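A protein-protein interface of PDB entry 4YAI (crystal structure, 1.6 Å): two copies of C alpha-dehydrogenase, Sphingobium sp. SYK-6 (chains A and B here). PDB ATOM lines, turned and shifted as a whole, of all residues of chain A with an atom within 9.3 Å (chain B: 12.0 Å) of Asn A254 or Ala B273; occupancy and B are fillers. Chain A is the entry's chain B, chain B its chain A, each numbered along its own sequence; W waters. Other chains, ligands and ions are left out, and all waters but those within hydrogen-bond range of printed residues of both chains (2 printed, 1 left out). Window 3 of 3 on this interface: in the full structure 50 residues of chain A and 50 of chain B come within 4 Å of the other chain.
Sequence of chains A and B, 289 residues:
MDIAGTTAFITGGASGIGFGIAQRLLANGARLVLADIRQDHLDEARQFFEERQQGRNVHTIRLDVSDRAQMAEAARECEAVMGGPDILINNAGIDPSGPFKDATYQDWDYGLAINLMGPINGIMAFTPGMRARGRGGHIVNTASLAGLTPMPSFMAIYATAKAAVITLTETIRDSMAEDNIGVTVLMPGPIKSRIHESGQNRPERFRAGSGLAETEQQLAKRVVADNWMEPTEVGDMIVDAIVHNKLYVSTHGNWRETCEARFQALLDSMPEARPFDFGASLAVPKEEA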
ATOM      1  N   LEU A 145      20.370   5.264  13.394  1.00  0.00           N
ATOM      2  CA  LEU A 145      19.166   6.078  13.485  1.00  0.00           C
ATOM      3  C   LEU A 145      19.450   7.480  12.923  1.00  0.00           C
ATOM      4  O   LEU A 145      18.526   8.212  12.563  1.00  0.00           O
ATOM      5  CB  LEU A 145      18.659   6.149  14.931  1.00  0.00           C
ATOM      6  CG  LEU A 145      17.996   4.868  15.439  1.00  0.00           C
ATOM      7  CD1 LEU A 145      17.847   4.883  16.958  1.00  0.00           C
ATOM      8  CD2 LEU A 145      16.642   4.638  14.783  1.00  0.00           C
ATOM      9  N   THR A 149      16.329   9.941  11.487  1.00  0.00           N
ATOM     10  CA  THR A 149      15.877  11.132  12.184  1.00  0.00           C
ATOM     11  C   THR A 149      16.630  12.358  11.624  1.00  0.00           C
ATOM     12  O   THR A 149      17.780  12.238  11.211  1.00  0.00           O
ATOM     13  CB  THR A 149      16.076  10.985  13.726  1.00  0.00           C
ATOM     14  OG1 THR A 149      15.265  11.945  14.420  1.00  0.00           O
ATOM     15  CG2 THR A 149      17.540  11.155  14.128  1.00  0.00           C
ATOM     16  N   MET A 187      19.838  -0.215  12.954  1.00  0.00           N
ATOM     17  CA  MET A 187      19.824   1.238  13.135  1.00  0.00           C
ATOM     18  C   MET A 187      20.020   1.557  14.610  1.00  0.00           C
ATOM     19  O   MET A 187      19.050   1.691  15.360  1.00  0.00           O
ATOM     20  CB  MET A 187      18.515   1.838  12.619  1.00  0.00           C
ATOM     21  CG  MET A 187      18.332   1.627  11.117  1.00  0.00           C
ATOM     22  SD  MET A 187      16.682   1.956  10.471  1.00  0.00           S
ATOM     23  CE  MET A 187      15.817   0.532  11.147  1.00  0.00           C
ATOM     24  N   PRO A 188      21.281   1.654  15.039  1.00  0.00           N
ATOM     25  CA  PRO A 188      21.471   1.898  16.470  1.00  0.00           C
ATOM     26  C   PRO A 188      21.356   3.349  16.882  1.00  0.00           C
ATOM     27  O   PRO A 188      21.578   4.266  16.078  1.00  0.00           O
ATOM     28  CB  PRO A 188      22.902   1.400  16.728  1.00  0.00           C
ATOM     29  CG  PRO A 188      23.319   0.671  15.495  1.00  0.00           C
ATOM     30  CD  PRO A 188      22.547   1.304  14.382  1.00  0.00           C
ATOM     31  N   GLY A 189      20.982   3.524  18.150  1.00  0.00           N
ATOM     32  CA  GLY A 189      21.226   4.733  18.907  1.00  0.00           C
ATOM     33  C   GLY A 189      22.600   4.595  19.544  1.00  0.00           C
ATOM     34  O   GLY A 189      23.421   3.816  19.064  1.00  0.00           O
ATOM     35  N   PRO A 190      22.856   5.329  20.637  1.00  0.00           N
ATOM     36  CA  PRO A 190      24.194   5.318  21.246  1.00  0.00           C
ATOM     37  C   PRO A 190      24.600   3.979  21.869  1.00  0.00           C
ATOM     38  O   PRO A 190      23.954   3.505  22.801  1.00  0.00           O
ATOM     39  CB  PRO A 190      24.095   6.401  22.328  1.00  0.00           C
ATOM     40  CG  PRO A 190      22.646   6.530  22.622  1.00  0.00           C
ATOM     41  CD  PRO A 190      21.938   6.246  21.333  1.00  0.00           C
ATOM     42  N   ASN A 227      25.731   5.115  30.282  1.00  0.00           N
ATOM     43  CA  ASN A 227      24.333   4.798  29.994  1.00  0.00           C
ATOM     44  C   ASN A 227      24.097   4.424  28.527  1.00  0.00           C
ATOM     45  O   ASN A 227      22.967   4.139  28.126  1.00  0.00           O
ATOM     46  CB  ASN A 227      23.431   5.974  30.382  1.00  0.00           C
ATOM     47  CG  ASN A 227      23.579   7.166  29.454  1.00  0.00           C
ATOM     48  OD1 ASN A 227      24.621   7.364  28.832  1.00  0.00           O
ATOM     49  ND2 ASN A 227      22.530   7.974  29.367  1.00  0.00           N
ATOM     50  N   MET A 229      24.306   1.833  25.380  1.00  0.00           N
ATOM     51  CA  MET A 229      23.990   0.416  25.351  1.00  0.00           C
ATOM     52  C   MET A 229      25.243  -0.441  25.185  1.00  0.00           C
ATOM     53  O   MET A 229      26.214  -0.021  24.557  1.00  0.00           O
ATOM     54  CB  MET A 229      23.007   0.141  24.220  1.00  0.00           C
ATOM     55  CG  MET A 229      22.584  -1.305  24.082  1.00  0.00           C
ATOM     56  SD  MET A 229      21.230  -1.475  22.913  1.00  0.00           S
ATOM     57  CE  MET A 229      19.874  -0.736  23.817  1.00  0.00           C
ATOM     58  N   SER A 250      15.982  -1.562  15.389  1.00  0.00           N
ATOM     59  CA  SER A 250      16.364  -0.317  16.043  1.00  0.00           C
ATOM     60  C   SER A 250      16.677  -0.589  17.506  1.00  0.00           C
ATOM     61  O   SER A 250      15.950  -1.333  18.171  1.00  0.00           O
ATOM     62  CB  SER A 250      15.254   0.720  15.931  1.00  0.00           C
ATOM     63  OG  SER A 250      14.993   1.027  14.575  1.00  0.00           O
ATOM     64  N   THR A 251      17.744   0.014  18.019  1.00  0.00           N
ATOM     65  CA  THR A 251      18.191  -0.299  19.375  1.00  0.00           C
ATOM     66  C   THR A 251      17.578   0.631  20.420  1.00  0.00           C
ATOM     67  O   THR A 251      17.489   0.271  21.600  1.00  0.00           O
ATOM     68  CB  THR A 251      19.719  -0.229  19.509  1.00  0.00           C
ATOM     69  OG1 THR A 251      20.156   1.119  19.321  1.00  0.00           O
ATOM     70  CG2 THR A 251      20.406  -1.151  18.506  1.00  0.00           C
ATOM     71  N   HIS A 252      17.154   1.815  19.981  1.00  0.00           N
ATOM     72  CA  HIS A 252      16.624   2.852  20.862  1.00  0.00           C
ATOM     73  C   HIS A 252      15.323   3.430  20.316  1.00  0.00           C
ATOM     74  O   HIS A 252      15.120   3.478  19.100  1.00  0.00           O
ATOM     75  CB  HIS A 252      17.632   3.995  21.041  1.00  0.00           C
ATOM     76  CG  HIS A 252      18.827   3.636  21.865  1.00  0.00           C
ATOM     77  ND1 HIS A 252      19.812   2.781  21.421  1.00  0.00           N
ATOM     78  CD2 HIS A 252      19.200   4.023  23.112  1.00  0.00           C
ATOM     79  CE1 HIS A 252      20.738   2.657  22.354  1.00  0.00           C
ATOM     80  NE2 HIS A 252      20.389   3.397  23.392  1.00  0.00           N
ATOM     81  N   GLY A 253      14.464   3.887  21.225  1.00  0.00           N
ATOM     82  CA  GLY A 253      13.209   4.522  20.852  1.00  0.00           C
ATOM     83  C   GLY A 253      13.186   6.029  21.044  1.00  0.00           C
ATOM     84  O   GLY A 253      12.151   6.666  20.869  1.00  0.00           O
ATOM     85  N   ASN A 254      14.332   6.608  21.380  1.00  0.00           N
ATOM     86  CA  ASN A 254      14.391   8.012  21.769  1.00  0.00           C
ATOM     87  C   ASN A 254      14.109   8.994  20.640  1.00  0.00           C
ATOM     88  O   ASN A 254      13.836  10.164  20.899  1.00  0.00           O
ATOM     89  CB  ASN A 254      15.760   8.313  22.368  1.00  0.00           C
ATOM     90  CG  ASN A 254      16.044   7.473  23.588  1.00  0.00           C
ATOM     91  OD1 ASN A 254      16.340   6.285  23.479  1.00  0.00           O
ATOM     92  ND2 ASN A 254      15.935   8.078  24.764  1.00  0.00           N
ATOM     93  N   TRP A 255      14.175   8.522  19.398  1.00  0.00           N
ATOM     94  CA  TRP A 255      13.951   9.377  18.238  1.00  0.00           C
ATOM     95  C   TRP A 255      12.647   9.013  17.520  1.00  0.00           C
ATOM     96  O   TRP A 255      12.453   9.355  16.360  1.00  0.00           O
ATOM     97  CB  TRP A 255      15.160   9.301  17.289  1.00  0.00           C
ATOM     98  CG  TRP A 255      16.367   9.956  17.909  1.00  0.00           C
ATOM     99  CD1 TRP A 255      16.708  11.275  17.840  1.00  0.00           C
ATOM    100  CD2 TRP A 255      17.364   9.326  18.717  1.00  0.00           C
ATOM    101  NE1 TRP A 255      17.861  11.506  18.558  1.00  0.00           N
ATOM    102  CE2 TRP A 255      18.282  10.323  19.106  1.00  0.00           C
ATOM    103  CE3 TRP A 255      17.568   8.015  19.157  1.00  0.00           C
ATOM    104  CZ2 TRP A 255      19.392  10.048  19.902  1.00  0.00           C
ATOM    105  CZ3 TRP A 255      18.669   7.745  19.952  1.00  0.00           C
ATOM    106  CH2 TRP A 255      19.566   8.756  20.315  1.00  0.00           C
ATOM    107  N   ARG A 256      11.737   8.345  18.227  1.00  0.00           N
ATOM    108  CA  ARG A 256      10.437   8.017  17.648  1.00  0.00           C
ATOM    109  C   ARG A 256       9.674   9.286  17.252  1.00  0.00           C
ATOM    110  O   ARG A 256       9.156   9.376  16.138  1.00  0.00           O
ATOM    111  CB  ARG A 256       9.593   7.188  18.621  1.00  0.00           C
ATOM    112  CG  ARG A 256       8.141   6.999  18.191  1.00  0.00           C
ATOM    113  CD  ARG A 256       7.358   6.212  19.240  1.00  0.00           C
ATOM    114  NE  ARG A 256       7.887   4.861  19.388  1.00  0.00           N
ATOM    115  CZ  ARG A 256       7.502   3.819  18.656  1.00  0.00           C
ATOM    116  NH1 ARG A 256       6.564   3.959  17.730  1.00  0.00           N
ATOM    117  NH2 ARG A 256       8.049   2.631  18.859  1.00  0.00           N
ATOM    118  N   GLU A 257       9.611  10.261  18.153  1.00  0.00           N
ATOM    119  CA  GLU A 257       8.830  11.472  17.891  1.00  0.00           C
ATOM    120  C   GLU A 257       9.471  12.360  16.837  1.00  0.00           C
ATOM    121  O   GLU A 257       8.766  13.006  16.065  1.00  0.00           O
ATOM    122  CB  GLU A 257       8.623  12.289  19.167  1.00  0.00           C
ATOM    123  CG  GLU A 257       7.475  11.792  20.021  1.00  0.00           C
ATOM    124  CD  GLU A 257       7.738  10.417  20.602  1.00  0.00           C
ATOM    125  OE1 GLU A 257       8.912  10.112  20.900  1.00  0.00           O
ATOM    126  OE2 GLU A 257       6.772   9.638  20.756  1.00  0.00           O
ATOM    127  N   THR A 258      10.799  12.409  16.806  1.00  0.00           N
ATOM    128  CA  THR A 258      11.487  13.231  15.821  1.00  0.00           C
ATOM    129  C   THR A 258      11.342  12.606  14.434  1.00  0.00           C
ATOM    130  O   THR A 258      11.151  13.313  13.448  1.00  0.00           O
ATOM    131  CB  THR A 258      12.984  13.434  16.166  1.00  0.00           C
ATOM    132  OG1 THR A 258      13.582  12.192  16.535  1.00  0.00           O
ATOM    133  CG2 THR A 258      13.130  14.408  17.322  1.00  0.00           C
ATOM    134  N   CYS A 259      11.401  11.278  14.365  1.00  0.00           N
ATOM    135  CA  CYS A 259      11.159  10.573  13.115  1.00  0.00           C
ATOM    136  C   CYS A 259       9.724  10.782  12.661  1.00  0.00           C
ATOM    137  O   CYS A 259       9.490  11.072  11.493  1.00  0.00           O
ATOM    138  CB  CYS A 259      11.448   9.081  13.256  1.00  0.00           C
ATOM    139  SG  CYS A 259      13.197   8.654  13.231  1.00  0.00           S
ATOM    140  N   GLU A 260       8.770  10.642  13.584  1.00  0.00           N
ATOM    141  CA  GLU A 260       7.365  10.879  13.262  1.00  0.00           C
ATOM    142  C   GLU A 260       7.145  12.263  12.656  1.00  0.00           C
ATOM    143  O   GLU A 260       6.401  12.411  11.685  1.00  0.00           O
ATOM    144  CB  GLU A 260       6.481  10.718  14.507  1.00  0.00           C
ATOM    145  CG  GLU A 260       6.161   9.283  14.848  1.00  0.00           C
ATOM    146  CD  GLU A 260       5.326   9.152  16.112  1.00  0.00           C
ATOM    147  OE1 GLU A 260       5.059  10.183  16.762  1.00  0.00           O
ATOM    148  OE2 GLU A 260       4.937   8.019  16.454  1.00  0.00           O
ATOM    149  N   LEU B 266       9.140   1.157  10.241  1.00  0.00           N
ATOM    150  CA  LEU B 266      10.322   1.742  10.872  1.00  0.00           C
ATOM    151  C   LEU B 266      10.053   2.099  12.332  1.00  0.00           C
ATOM    152  O   LEU B 266      10.837   1.760  13.218  1.00  0.00           O
ATOM    153  CB  LEU B 266      10.783   2.984  10.103  1.00  0.00           C
ATOM    154  CG  LEU B 266      11.401   2.668   8.732  1.00  0.00           C
ATOM    155  CD1 LEU B 266      11.477   3.874   7.825  1.00  0.00           C
ATOM    156  CD2 LEU B 266      12.801   2.061   8.886  1.00  0.00           C
ATOM    157  N   LEU B 267       8.945   2.790  12.583  1.00  0.00           N
ATOM    158  CA  LEU B 267       8.589   3.179  13.948  1.00  0.00           C
ATOM    159  C   LEU B 267       8.342   1.953  14.825  1.00  0.00           C
ATOM    160  O   LEU B 267       8.722   1.928  16.000  1.00  0.00           O
ATOM    161  CB  LEU B 267       7.356   4.085  13.935  1.00  0.00           C
ATOM    162  CG  LEU B 267       7.543   5.436  13.232  1.00  0.00           C
ATOM    163  CD1 LEU B 267       6.210   6.142  13.046  1.00  0.00           C
ATOM    164  CD2 LEU B 267       8.507   6.339  13.993  1.00  0.00           C
ATOM    165  N   ASP B 268       7.724   0.930  14.251  1.00  0.00           N
ATOM    166  CA  ASP B 268       7.404  -0.279  15.003  1.00  0.00           C
ATOM    167  C   ASP B 268       8.660  -1.017  15.457  1.00  0.00           C
ATOM    168  O   ASP B 268       8.621  -1.764  16.441  1.00  0.00           O
ATOM    169  CB  ASP B 268       6.534  -1.216  14.166  1.00  0.00           C
ATOM    170  CG  ASP B 268       5.088  -0.744  14.063  1.00  0.00           C
ATOM    171  OD1 ASP B 268       4.700   0.207  14.776  1.00  0.00           O
ATOM    172  OD2 ASP B 268       4.338  -1.335  13.258  1.00  0.00           O
ATOM    173  N   SER B 269       9.771  -0.812  14.750  1.00  0.00           N
ATOM    174  CA  SER B 269      11.021  -1.476  15.110  1.00  0.00           C
ATOM    175  C   SER B 269      11.667  -0.824  16.328  1.00  0.00           C
ATOM    176  O   SER B 269      12.614  -1.363  16.896  1.00  0.00           O
ATOM    177  CB  SER B 269      12.008  -1.468  13.936  1.00  0.00           C
ATOM    178  OG  SER B 269      12.673  -0.222  13.805  1.00  0.00           O
ATOM    179  N   MET B 270      11.156   0.334  16.729  1.00  0.00           N
ATOM    180  CA  MET B 270      11.762   1.078  17.829  1.00  0.00           C
ATOM    181  C   MET B 270      11.144   0.677  19.159  1.00  0.00           C
ATOM    182  O   MET B 270       9.922   0.639  19.284  1.00  0.00           O
ATOM    183  CB  MET B 270      11.599   2.578  17.619  1.00  0.00           C
ATOM    184  CG  MET B 270      12.212   3.072  16.328  1.00  0.00           C
ATOM    185  SD  MET B 270      11.893   4.822  16.035  1.00  0.00           S
ATOM    186  CE  MET B 270      12.605   5.002  14.418  1.00  0.00           C
ATOM    187  N   PRO B 271      11.988   0.377  20.154  1.00  0.00           N
ATOM    188  CA  PRO B 271      11.443  -0.010  21.458  1.00  0.00           C
ATOM    189  C   PRO B 271      10.884   1.189  22.201  1.00  0.00           C
ATOM    190  O   PRO B 271      11.061   2.318  21.760  1.00  0.00           O
ATOM    191  CB  PRO B 271      12.655  -0.586  22.186  1.00  0.00           C
ATOM    192  CG  PRO B 271      13.815   0.125  21.600  1.00  0.00           C
ATOM    193  CD  PRO B 271      13.461   0.384  20.157  1.00  0.00           C
ATOM    194  N   GLU B 272      10.206   0.946  23.316  1.00  0.00           N
ATOM    195  CA  GLU B 272       9.816   2.041  24.191  1.00  0.00           C
ATOM    196  C   GLU B 272      11.072   2.729  24.716  1.00  0.00           C
ATOM    197  O   GLU B 272      11.954   2.076  25.274  1.00  0.00           O
ATOM    198  CB  GLU B 272       8.961   1.538  25.351  1.00  0.00           C
ATOM    199  CG  GLU B 272       8.591   2.625  26.339  1.00  0.00           C
ATOM    200  CD  GLU B 272       8.151   2.072  27.676  1.00  0.00           C
ATOM    201  OE1 GLU B 272       8.252   2.809  28.680  1.00  0.00           O
ATOM    202  OE2 GLU B 272       7.708   0.904  27.726  1.00  0.00           O
ATOM    203  N   ALA B 273      11.162   4.040  24.526  1.00  0.00           N
ATOM    204  CA  ALA B 273      12.300   4.796  25.037  1.00  0.00           C
ATOM    205  C   ALA B 273      12.287   4.815  26.564  1.00  0.00           C
ATOM    206  O   ALA B 273      13.301   4.549  27.211  1.00  0.00           O
ATOM    207  CB  ALA B 273      12.293   6.213  24.485  1.00  0.00           C
HETATM  208  O   HOH W   1      14.032  -3.570  16.587  1.00  0.00           O
HETATM  209  O   HOH W   2       5.081   2.112  16.473  1.00  0.00           O
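Water W2 bridges OD1 of Asp B268 (2.6 Å) and NH1 of Arg A256 (2.7 Å). Water W1 bridges the backbone carbonyl oxygen (O) of Ser B269 (2.6 Å) and the backbone NH (N) of Ser A250 (3.0 Å).
Of the 8 printed residues of chain B, 5 touch a printed residue of chain A. Printed residues of chain B that touch a printed residue of chain A: Leu B267, Ser B269, Met B270, Pro B271 and Ala B273. Hydrophobic or aromatic side chains of chain B within 4 Å of the printed part of chain A: Leu B267, Met B270, Pro B271 and Ala B273. Along chain A the printed residues that touch a printed residue of chain B span positions 250 to 260. Among the printed residues, 13 pairs touch across the chains.
Ser A250 touches Met B270 (CB to CG, 3.9 Å). O of Ser A250 touches CD of Pro B271, 3.6 Å away. CG of Pro B271 touches O of Thr A251, 3.7 Å away. CB of Met B270 touches O of His A252 (3.9 Å). C of His A252 touches CD of Pro B271, at 3.6 Å. CA of Gly A253 touches O of Pro B271, 3.2 Å away. Gly A253 touches Ala B273. Asn A254 touches Ala B273. Cys A259 touches Met B270 (SG to CE, 3.9 Å). Glu A260 touches Leu B267 (CG to CD1, 3.6 Å).
O of Leu B267 lies within hydrogen-bond range of NH2 of Arg A256 (3.0 Å). The side-chain hydroxyl (OG) of Ser B269 lies within hydrogen-bond range of the side-chain hydroxyl (OG) of Ser A250, at 2.7 Å. O of Met B270 sits at hydrogen-bond distance from NH2 of Arg A256 (2.8 Å).
Pro A188 touches none of the printed residues of chain B. Of the printed residues of chain B, His A252 touches Met B270 (3.9 Å) and Pro B271 (3.6 Å). Gly A253 touches just these residues of chain B: Pro B271 (3.2 Å) and Ala B273 (3.6 Å). Of chain B, only Ala B273 comes within 4 Å of Asn A254. No residue of chain B comes within 4 Å of Trp A255. Printed residues of chain A within 4 Å of Leu B267: Arg A256 (3.0 Å) and Glu A260 (3.6 Å). Asp B268 touches none of the printed residues of chain A. Printed residues of chain A within 4 Å of Met B270: Ser A250 (3.9 Å), His A252 (3.9 Å), Arg A256 (2.8 Å) and Cys A259 (3.9 Å). Ala B273 touches just these residues of chain A: Gly A253 and Asn A254. The nearest residue of chain B that does not touch Asn A254 is Pro B271 (5.4 Å). The nearest printed residue of chain A that does not touch Ser B269 is Met A187 (4.2 Å).
OG1 of Thr A251 sits at hydrogen-bond distance from ND1 of His A252 (2.7 Å). The backbone carbonyl oxygen (O) of Leu B266 lies within hydrogen-bond range of the side-chain hydroxyl (OG) of Ser B269, at 2.8 Å. SG of Cys A259 lies close to O of Trp A255, at 3.3 Å. OG1 of Thr A251 is in hydrogen-bond range of N of Gly A189 (2.8 Å). The backbone NH (N) of Thr A251 lies within hydrogen-bond range of the backbone carbonyl oxygen (O) of Met A187, at 3.4 Å.
No position is printed for both chains. Of the 13 pairs that touch across the chains among the printed residues, none has its exchanged pair printed and touching as well.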
